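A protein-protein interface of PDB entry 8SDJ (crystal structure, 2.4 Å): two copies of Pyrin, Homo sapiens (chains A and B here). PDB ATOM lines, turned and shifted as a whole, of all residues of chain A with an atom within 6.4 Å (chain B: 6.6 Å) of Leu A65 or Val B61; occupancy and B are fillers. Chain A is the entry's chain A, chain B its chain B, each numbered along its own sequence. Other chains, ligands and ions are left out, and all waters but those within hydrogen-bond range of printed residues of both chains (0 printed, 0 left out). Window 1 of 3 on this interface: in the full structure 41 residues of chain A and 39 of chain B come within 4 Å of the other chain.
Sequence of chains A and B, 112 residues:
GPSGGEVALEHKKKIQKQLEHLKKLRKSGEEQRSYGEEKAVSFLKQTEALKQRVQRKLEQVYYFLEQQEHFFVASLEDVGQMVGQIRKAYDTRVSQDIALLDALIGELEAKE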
ATOM      1  N   GLN A  60     -19.185 -15.368 -20.772  1.00  0.00           N
ATOM      2  CA  GLN A  60     -19.493 -13.953 -20.825  1.00  0.00           C
ATOM      3  C   GLN A  60     -18.925 -13.183 -19.628  1.00  0.00           C
ATOM      4  O   GLN A  60     -18.480 -12.048 -19.799  1.00  0.00           O
ATOM      5  CB  GLN A  60     -20.997 -13.799 -20.913  1.00  0.00           C
ATOM      6  CG  GLN A  60     -21.502 -14.255 -22.270  1.00  0.00           C
ATOM      7  CD  GLN A  60     -23.006 -14.262 -22.318  1.00  0.00           C
ATOM      8  OE1 GLN A  60     -23.672 -14.562 -21.327  1.00  0.00           O
ATOM      9  NE2 GLN A  60     -23.552 -13.923 -23.478  1.00  0.00           N
ATOM     10  N   VAL A  61     -18.935 -13.790 -18.425  1.00  0.00           N
ATOM     11  CA  VAL A  61     -18.566 -13.123 -17.175  1.00  0.00           C
ATOM     12  C   VAL A  61     -17.062 -12.832 -17.166  1.00  0.00           C
ATOM     13  O   VAL A  61     -16.631 -11.707 -16.889  1.00  0.00           O
ATOM     14  CB  VAL A  61     -18.954 -13.963 -15.935  1.00  0.00           C
ATOM     15  CG1 VAL A  61     -18.542 -13.309 -14.618  1.00  0.00           C
ATOM     16  CG2 VAL A  61     -20.437 -14.279 -15.906  1.00  0.00           C
ATOM     17  N   TYR A  62     -16.275 -13.889 -17.402  1.00  0.00           N
ATOM     18  CA  TYR A  62     -14.835 -13.852 -17.591  1.00  0.00           C
ATOM     19  C   TYR A  62     -14.411 -12.697 -18.502  1.00  0.00           C
ATOM     20  O   TYR A  62     -13.560 -11.915 -18.113  1.00  0.00           O
ATOM     21  CB  TYR A  62     -14.319 -15.194 -18.126  1.00  0.00           C
ATOM     22  CG  TYR A  62     -12.976 -15.557 -17.557  1.00  0.00           C
ATOM     23  CD1 TYR A  62     -11.806 -15.103 -18.154  1.00  0.00           C
ATOM     24  CD2 TYR A  62     -12.879 -16.293 -16.382  1.00  0.00           C
ATOM     25  CE1 TYR A  62     -10.564 -15.395 -17.618  1.00  0.00           C
ATOM     26  CE2 TYR A  62     -11.643 -16.592 -15.828  1.00  0.00           C
ATOM     27  CZ  TYR A  62     -10.486 -16.139 -16.450  1.00  0.00           C
ATOM     28  OH  TYR A  62      -9.266 -16.422 -15.915  1.00  0.00           O
ATOM     29  N   TYR A  63     -14.949 -12.620 -19.722  1.00  0.00           N
ATOM     30  CA  TYR A  63     -14.545 -11.580 -20.642  1.00  0.00           C
ATOM     31  C   TYR A  63     -14.926 -10.212 -20.074  1.00  0.00           C
ATOM     32  O   TYR A  63     -14.202  -9.240 -20.285  1.00  0.00           O
ATOM     33  CB  TYR A  63     -15.022 -11.872 -22.075  1.00  0.00           C
ATOM     34  CG  TYR A  63     -15.277 -10.651 -22.927  1.00  0.00           C
ATOM     35  CD1 TYR A  63     -14.225  -9.932 -23.487  1.00  0.00           C
ATOM     36  CD2 TYR A  63     -16.573 -10.200 -23.164  1.00  0.00           C
ATOM     37  CE1 TYR A  63     -14.460  -8.799 -24.257  1.00  0.00           C
ATOM     38  CE2 TYR A  63     -16.824  -9.063 -23.918  1.00  0.00           C
ATOM     39  CZ  TYR A  63     -15.762  -8.366 -24.468  1.00  0.00           C
ATOM     40  OH  TYR A  63     -16.025  -7.254 -25.208  1.00  0.00           O
ATOM     41  N   PHE A  64     -16.029 -10.161 -19.311  1.00  0.00           N
ATOM     42  CA  PHE A  64     -16.518  -8.941 -18.681  1.00  0.00           C
ATOM     43  C   PHE A  64     -15.533  -8.438 -17.620  1.00  0.00           C
ATOM     44  O   PHE A  64     -15.302  -7.240 -17.492  1.00  0.00           O
ATOM     45  CB  PHE A  64     -17.946  -9.123 -18.135  1.00  0.00           C
ATOM     46  CG  PHE A  64     -18.443  -7.954 -17.321  1.00  0.00           C
ATOM     47  CD1 PHE A  64     -18.987  -6.839 -17.945  1.00  0.00           C
ATOM     48  CD2 PHE A  64     -18.291  -7.927 -15.940  1.00  0.00           C
ATOM     49  CE1 PHE A  64     -19.402  -5.737 -17.208  1.00  0.00           C
ATOM     50  CE2 PHE A  64     -18.706  -6.824 -15.203  1.00  0.00           C
ATOM     51  CZ  PHE A  64     -19.258  -5.731 -15.833  1.00  0.00           C
ATOM     52  N   LEU A  65     -14.939  -9.363 -16.867  1.00  0.00           N
ATOM     53  CA  LEU A  65     -13.937  -9.003 -15.896  1.00  0.00           C
ATOM     54  C   LEU A  65     -12.702  -8.440 -16.602  1.00  0.00           C
ATOM     55  O   LEU A  65     -12.149  -7.423 -16.188  1.00  0.00           O
ATOM     56  CB  LEU A  65     -13.615 -10.252 -15.078  1.00  0.00           C
ATOM     57  CG  LEU A  65     -14.652 -10.615 -14.012  1.00  0.00           C
ATOM     58  CD1 LEU A  65     -14.165 -11.764 -13.142  1.00  0.00           C
ATOM     59  CD2 LEU A  65     -15.036  -9.424 -13.142  1.00  0.00           C
ATOM     60  N   GLU A  66     -12.277  -9.097 -17.683  1.00  0.00           N
ATOM     61  CA  GLU A  66     -11.101  -8.686 -18.436  1.00  0.00           C
ATOM     62  C   GLU A  66     -11.248  -7.215 -18.821  1.00  0.00           C
ATOM     63  O   GLU A  66     -10.366  -6.404 -18.556  1.00  0.00           O
ATOM     64  CB  GLU A  66     -10.953  -9.576 -19.671  1.00  0.00           C
ATOM     65  CG  GLU A  66      -9.565  -9.614 -20.268  1.00  0.00           C
ATOM     66  CD  GLU A  66      -9.568 -10.125 -21.708  1.00  0.00           C
ATOM     67  OE1 GLU A  66      -8.481 -10.519 -22.211  1.00  0.00           O
ATOM     68  OE2 GLU A  66     -10.666 -10.128 -22.337  1.00  0.00           O
ATOM     69  N   GLN A  67     -12.383  -6.881 -19.432  1.00  0.00           N
ATOM     70  CA  GLN A  67     -12.670  -5.539 -19.900  1.00  0.00           C
ATOM     71  C   GLN A  67     -12.662  -4.535 -18.736  1.00  0.00           C
ATOM     72  O   GLN A  67     -12.247  -3.386 -18.903  1.00  0.00           O
ATOM     73  CB  GLN A  67     -14.019  -5.538 -20.625  1.00  0.00           C
ATOM     74  CG  GLN A  67     -13.935  -5.883 -22.111  1.00  0.00           C
ATOM     75  CD  GLN A  67     -14.776  -4.923 -22.920  1.00  0.00           C
ATOM     76  OE1 GLN A  67     -15.021  -3.792 -22.521  1.00  0.00           O
ATOM     77  NE2 GLN A  67     -15.239  -5.369 -24.073  1.00  0.00           N
ATOM     78  N   GLN A  68     -13.118  -4.956 -17.549  1.00  0.00           N
ATOM     79  CA  GLN A  68     -13.124  -4.055 -16.410  1.00  0.00           C
ATOM     80  C   GLN A  68     -11.711  -3.899 -15.841  1.00  0.00           C
ATOM     81  O   GLN A  68     -11.231  -2.787 -15.659  1.00  0.00           O
ATOM     82  CB  GLN A  68     -14.185  -4.466 -15.373  1.00  0.00           C
ATOM     83  CG  GLN A  68     -15.600  -4.482 -15.941  1.00  0.00           C
ATOM     84  CD  GLN A  68     -16.000  -3.159 -16.538  1.00  0.00           C
ATOM     85  OE1 GLN A  68     -16.689  -3.088 -17.557  1.00  0.00           O
ATOM     86  NE2 GLN A  68     -15.569  -2.089 -15.892  1.00  0.00           N
ATOM     87  N   GLU A  69     -11.028  -5.016 -15.595  1.00  0.00           N
ATOM     88  CA  GLU A  69      -9.604  -4.950 -15.338  1.00  0.00           C
ATOM     89  C   GLU A  69      -8.927  -3.984 -16.322  1.00  0.00           C
ATOM     90  O   GLU A  69      -8.196  -3.104 -15.915  1.00  0.00           O
ATOM     91  CB  GLU A  69      -9.020  -6.355 -15.343  1.00  0.00           C
ATOM     92  CG  GLU A  69      -7.561  -6.395 -14.928  1.00  0.00           C
ATOM     93  CD  GLU A  69      -7.044  -7.812 -14.763  1.00  0.00           C
ATOM     94  OE1 GLU A  69      -7.776  -8.752 -15.143  1.00  0.00           O
ATOM     95  OE2 GLU A  69      -5.926  -7.984 -14.228  1.00  0.00           O
ATOM     96  N   HIS A  70      -9.221  -4.092 -17.617  1.00  0.00           N
ATOM     97  CA  HIS A  70      -8.580  -3.200 -18.563  1.00  0.00           C
ATOM     98  C   HIS A  70      -8.954  -1.747 -18.279  1.00  0.00           C
ATOM     99  O   HIS A  70      -8.097  -0.858 -18.272  1.00  0.00           O
ATOM    100  CB  HIS A  70      -8.873  -3.605 -20.017  1.00  0.00           C
ATOM    101  CG  HIS A  70      -8.145  -2.775 -21.028  1.00  0.00           C
ATOM    102  ND1 HIS A  70      -6.817  -3.024 -21.386  1.00  0.00           N
ATOM    103  CD2 HIS A  70      -8.546  -1.700 -21.756  1.00  0.00           C
ATOM    104  CE1 HIS A  70      -6.447  -2.141 -22.300  1.00  0.00           C
ATOM    105  NE2 HIS A  70      -7.490  -1.308 -22.542  1.00  0.00           N
ATOM    106  N   ARG B  56      -4.776  -8.450  -7.904  1.00  0.00           N
ATOM    107  CA  ARG B  56      -4.724  -9.578  -6.988  1.00  0.00           C
ATOM    108  C   ARG B  56      -6.150 -10.063  -6.684  1.00  0.00           C
ATOM    109  O   ARG B  56      -6.396 -11.264  -6.669  1.00  0.00           O
ATOM    110  CB  ARG B  56      -3.828  -9.194  -5.799  1.00  0.00           C
ATOM    111  CG  ARG B  56      -4.266  -9.661  -4.413  1.00  0.00           C
ATOM    112  CD  ARG B  56      -3.467  -8.996  -3.295  1.00  0.00           C
ATOM    113  NE  ARG B  56      -2.036  -8.988  -3.607  1.00  0.00           N
ATOM    114  CZ  ARG B  56      -1.226  -7.923  -3.642  1.00  0.00           C
ATOM    115  NH1 ARG B  56      -1.673  -6.714  -3.339  1.00  0.00           N
ATOM    116  NH2 ARG B  56       0.047  -8.084  -3.961  1.00  0.00           N
ATOM    117  N   LYS B  57      -7.098  -9.134  -6.516  1.00  0.00           N
ATOM    118  CA  LYS B  57      -8.488  -9.496  -6.288  1.00  0.00           C
ATOM    119  C   LYS B  57      -9.035 -10.217  -7.517  1.00  0.00           C
ATOM    120  O   LYS B  57      -9.519 -11.349  -7.411  1.00  0.00           O
ATOM    121  CB  LYS B  57      -9.401  -8.292  -5.979  1.00  0.00           C
ATOM    122  CG  LYS B  57      -9.519  -7.862  -4.520  1.00  0.00           C
ATOM    123  CD  LYS B  57      -9.687  -9.036  -3.569  1.00  0.00           C
ATOM    124  CE  LYS B  57      -8.919  -8.838  -2.282  1.00  0.00           C
ATOM    125  NZ  LYS B  57      -9.393  -9.755  -1.224  1.00  0.00           N
ATOM    126  N   LEU B  58      -8.977  -9.540  -8.674  1.00  0.00           N
ATOM    127  CA  LEU B  58      -9.606 -10.079  -9.859  1.00  0.00           C
ATOM    128  C   LEU B  58      -8.992 -11.445 -10.154  1.00  0.00           C
ATOM    129  O   LEU B  58      -9.694 -12.373 -10.547  1.00  0.00           O
ATOM    130  CB  LEU B  58      -9.478  -9.079 -11.007  1.00  0.00           C
ATOM    131  CG  LEU B  58     -10.457  -7.902 -10.943  1.00  0.00           C
ATOM    132  CD1 LEU B  58     -10.081  -6.798 -11.921  1.00  0.00           C
ATOM    133  CD2 LEU B  58     -11.881  -8.339 -11.180  1.00  0.00           C
ATOM    134  N   GLU B  59      -7.706 -11.603  -9.837  1.00  0.00           N
ATOM    135  CA  GLU B  59      -7.083 -12.900 -10.000  1.00  0.00           C
ATOM    136  C   GLU B  59      -7.853 -13.944  -9.176  1.00  0.00           C
ATOM    137  O   GLU B  59      -8.175 -15.012  -9.703  1.00  0.00           O
ATOM    138  CB  GLU B  59      -5.568 -12.801  -9.791  1.00  0.00           C
ATOM    139  CG  GLU B  59      -4.775 -12.752 -11.097  1.00  0.00           C
ATOM    140  CD  GLU B  59      -4.513 -11.387 -11.728  1.00  0.00           C
ATOM    141  OE1 GLU B  59      -4.984 -11.143 -12.867  1.00  0.00           O
ATOM    142  OE2 GLU B  59      -3.806 -10.578 -11.095  1.00  0.00           O
ATOM    143  N   GLN B  60      -8.205 -13.584  -7.924  1.00  0.00           N
ATOM    144  CA  GLN B  60      -8.867 -14.469  -6.979  1.00  0.00           C
ATOM    145  C   GLN B  60     -10.262 -14.840  -7.493  1.00  0.00           C
ATOM    146  O   GLN B  60     -10.763 -15.927  -7.219  1.00  0.00           O
ATOM    147  CB  GLN B  60      -8.892 -13.827  -5.584  1.00  0.00           C
ATOM    148  CG  GLN B  60      -7.527 -13.762  -4.891  1.00  0.00           C
ATOM    149  CD  GLN B  60      -7.503 -13.121  -3.519  1.00  0.00           C
ATOM    150  OE1 GLN B  60      -8.218 -12.157  -3.232  1.00  0.00           O
ATOM    151  NE2 GLN B  60      -6.638 -13.631  -2.656  1.00  0.00           N
ATOM    152  N   VAL B  61     -10.888 -13.934  -8.248  1.00  0.00           N
ATOM    153  CA  VAL B  61     -12.239 -14.146  -8.747  1.00  0.00           C
ATOM    154  C   VAL B  61     -12.181 -15.078  -9.952  1.00  0.00           C
ATOM    155  O   VAL B  61     -12.941 -16.042 -10.004  1.00  0.00           O
ATOM    156  CB  VAL B  61     -12.917 -12.811  -9.107  1.00  0.00           C
ATOM    157  CG1 VAL B  61     -14.377 -12.976  -9.492  1.00  0.00           C
ATOM    158  CG2 VAL B  61     -12.773 -11.811  -7.973  1.00  0.00           C
ATOM    159  N   TYR B  62     -11.254 -14.789 -10.878  1.00  0.00           N
ATOM    160  CA  TYR B  62     -10.958 -15.605 -12.046  1.00  0.00           C
ATOM    161  C   TYR B  62     -10.840 -17.083 -11.680  1.00  0.00           C
ATOM    162  O   TYR B  62     -11.457 -17.925 -12.332  1.00  0.00           O
ATOM    163  CB  TYR B  62      -9.579 -15.278 -12.614  1.00  0.00           C
ATOM    164  CG  TYR B  62      -9.478 -14.149 -13.606  1.00  0.00           C
ATOM    165  CD1 TYR B  62     -10.602 -13.491 -14.097  1.00  0.00           C
ATOM    166  CD2 TYR B  62      -8.231 -13.766 -14.091  1.00  0.00           C
ATOM    167  CE1 TYR B  62     -10.480 -12.468 -15.029  1.00  0.00           C
ATOM    168  CE2 TYR B  62      -8.095 -12.746 -15.019  1.00  0.00           C
ATOM    169  CZ  TYR B  62      -9.224 -12.094 -15.489  1.00  0.00           C
ATOM    170  OH  TYR B  62      -9.084 -11.086 -16.401  1.00  0.00           O
ATOM    171  N   TYR B  63      -9.974 -17.391 -10.703  1.00  0.00           N
ATOM    172  CA  TYR B  63      -9.650 -18.758 -10.338  1.00  0.00           C
ATOM    173  C   TYR B  63     -10.822 -19.374  -9.565  1.00  0.00           C
ATOM    174  O   TYR B  63     -11.009 -20.581  -9.621  1.00  0.00           O
ATOM    175  CB  TYR B  63      -8.264 -18.862  -9.672  1.00  0.00           C
ATOM    176  CG  TYR B  63      -8.118 -19.989  -8.666  1.00  0.00           C
ATOM    177  CD1 TYR B  63      -7.931 -21.302  -9.085  1.00  0.00           C
ATOM    178  CD2 TYR B  63      -8.202 -19.760  -7.291  1.00  0.00           C
ATOM    179  CE1 TYR B  63      -7.831 -22.345  -8.172  1.00  0.00           C
ATOM    180  CE2 TYR B  63      -8.134 -20.793  -6.369  1.00  0.00           C
ATOM    181  CZ  TYR B  63      -7.952 -22.090  -6.813  1.00  0.00           C
ATOM    182  OH  TYR B  63      -7.870 -23.095  -5.894  1.00  0.00           O
ATOM    183  N   PHE B  64     -11.637 -18.556  -8.883  1.00  0.00           N
ATOM    184  CA  PHE B  64     -12.813 -19.052  -8.177  1.00  0.00           C
ATOM    185  C   PHE B  64     -13.886 -19.459  -9.189  1.00  0.00           C
ATOM    186  O   PHE B  64     -14.556 -20.473  -9.021  1.00  0.00           O
ATOM    187  CB  PHE B  64     -13.327 -18.008  -7.173  1.00  0.00           C
ATOM    188  CG  PHE B  64     -14.628 -18.351  -6.484  1.00  0.00           C
ATOM    189  CD1 PHE B  64     -15.853 -17.978  -7.032  1.00  0.00           C
ATOM    190  CD2 PHE B  64     -14.633 -19.034  -5.271  1.00  0.00           C
ATOM    191  CE1 PHE B  64     -17.046 -18.327  -6.413  1.00  0.00           C
ATOM    192  CE2 PHE B  64     -15.829 -19.363  -4.637  1.00  0.00           C
ATOM    193  CZ  PHE B  64     -17.035 -18.999  -5.207  1.00  0.00           C
ATOM    194  N   LEU B  65     -14.035 -18.671 -10.260  1.00  0.00           N
ATOM    195  CA  LEU B  65     -14.965 -19.040 -11.294  1.00  0.00           C
ATOM    196  C   LEU B  65     -14.492 -20.319 -11.994  1.00  0.00           C
ATOM    197  O   LEU B  65     -15.271 -21.056 -12.582  1.00  0.00           O
ATOM    198  CB  LEU B  65     -15.090 -17.860 -12.257  1.00  0.00           C
ATOM    199  CG  LEU B  65     -15.944 -16.692 -11.756  1.00  0.00           C
ATOM    200  CD1 LEU B  65     -16.448 -15.839 -12.905  1.00  0.00           C
ATOM    201  CD2 LEU B  65     -17.115 -17.155 -10.895  1.00  0.00           C
ATOM    202  N   GLU B  66     -13.198 -20.587 -11.970  1.00  0.00           N
ATOM    203  CA  GLU B  66     -12.683 -21.740 -12.694  1.00  0.00           C
ATOM    204  C   GLU B  66     -12.984 -23.014 -11.897  1.00  0.00           C
ATOM    205  O   GLU B  66     -13.503 -23.995 -12.429  1.00  0.00           O
ATOM    206  CB  GLU B  66     -11.200 -21.498 -12.989  1.00  0.00           C
ATOM    207  CG  GLU B  66     -10.531 -22.587 -13.798  1.00  0.00           C
ATOM    208  CD  GLU B  66      -9.013 -22.509 -13.721  1.00  0.00           C
ATOM    209  OE1 GLU B  66      -8.340 -23.022 -14.668  1.00  0.00           O
ATOM    210  OE2 GLU B  66      -8.507 -21.926 -12.714  1.00  0.00           O
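OE1 of Glu A69 lies within hydrogen-bond range of OH of Tyr B62.
CG1 of Val A61 touches CD1 of Leu B65 (3.7 Å). CG of Tyr B62 touches OH of Tyr A62 (3.2 Å). CD2 of Leu B58 touches CD2 of Leu A65, at 3.9 Å. Leu A65 touches Val B61 (CD1 to CG1, 3.9 Å). CE1 of Tyr B62 touches CB of Leu A65, 3.8 Å away. CA of Glu A66 touches OH of Tyr B62 (3.7 Å). Glu A69 touches Leu B58. OE1 of Glu B59 touches OE2 of Glu A69 (3.6 Å).
Of chain B, only Leu B58, Val B61 and Tyr B62 come within 4 Å of Leu A65. Val B61 touches just one residue of chain A: Leu A65. Of the printed residues of chain A, Leu B58 touches Leu A65 (3.9 Å) and Glu A69 (3.6 Å). Printed residues of chain A within 4 Å of Tyr B62: Tyr A62 (3.2 Å), Leu A65 (3.8 Å), Glu A66 (3.7 Å) and Glu A69 (3.0 Å). Of the printed residues of chain B, Tyr A62 touches Tyr B62 (3.2 Å). Of the printed residues of chain A, Glu B59 touches Glu A69 (3.6 Å). The nearest residue of chain A that does not touch Val B61 is Tyr A62 (6.0 Å).
Printed residues of chain A that touch a printed residue of chain B: Val A61, Tyr A62, Leu A65, Glu A66 and Glu A69. Of the 11 printed residues of chain B, 5 touch a printed residue of chain A. Hydrophobic or aromatic side chains of chain B within 4 Å of the printed part of chain A: Leu B58, Val B61, Tyr B62 and Leu B65. Among the printed residues, 9 pairs touch across the chains.
Val A61 touches Leu B65, and with the chains exchanged Leu A65 touches Val B61. Tyr A62 touches its own counterpart, Tyr B62. Leu A65 touches Tyr B62, but with the chains exchanged Tyr A62 does not touch Leu B65 (4.9 Å). Glu A66 touches Tyr B62, but with the chains exchanged Tyr A62 does not touch Glu B66 (5.7 Å). Positions printed for both chains: 60, 61, 62, 63, 64, 65 and 66. Of the 9 pairs that touch across the chains among the printed residues, 3 have their exchanged pair printed and touching as well.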
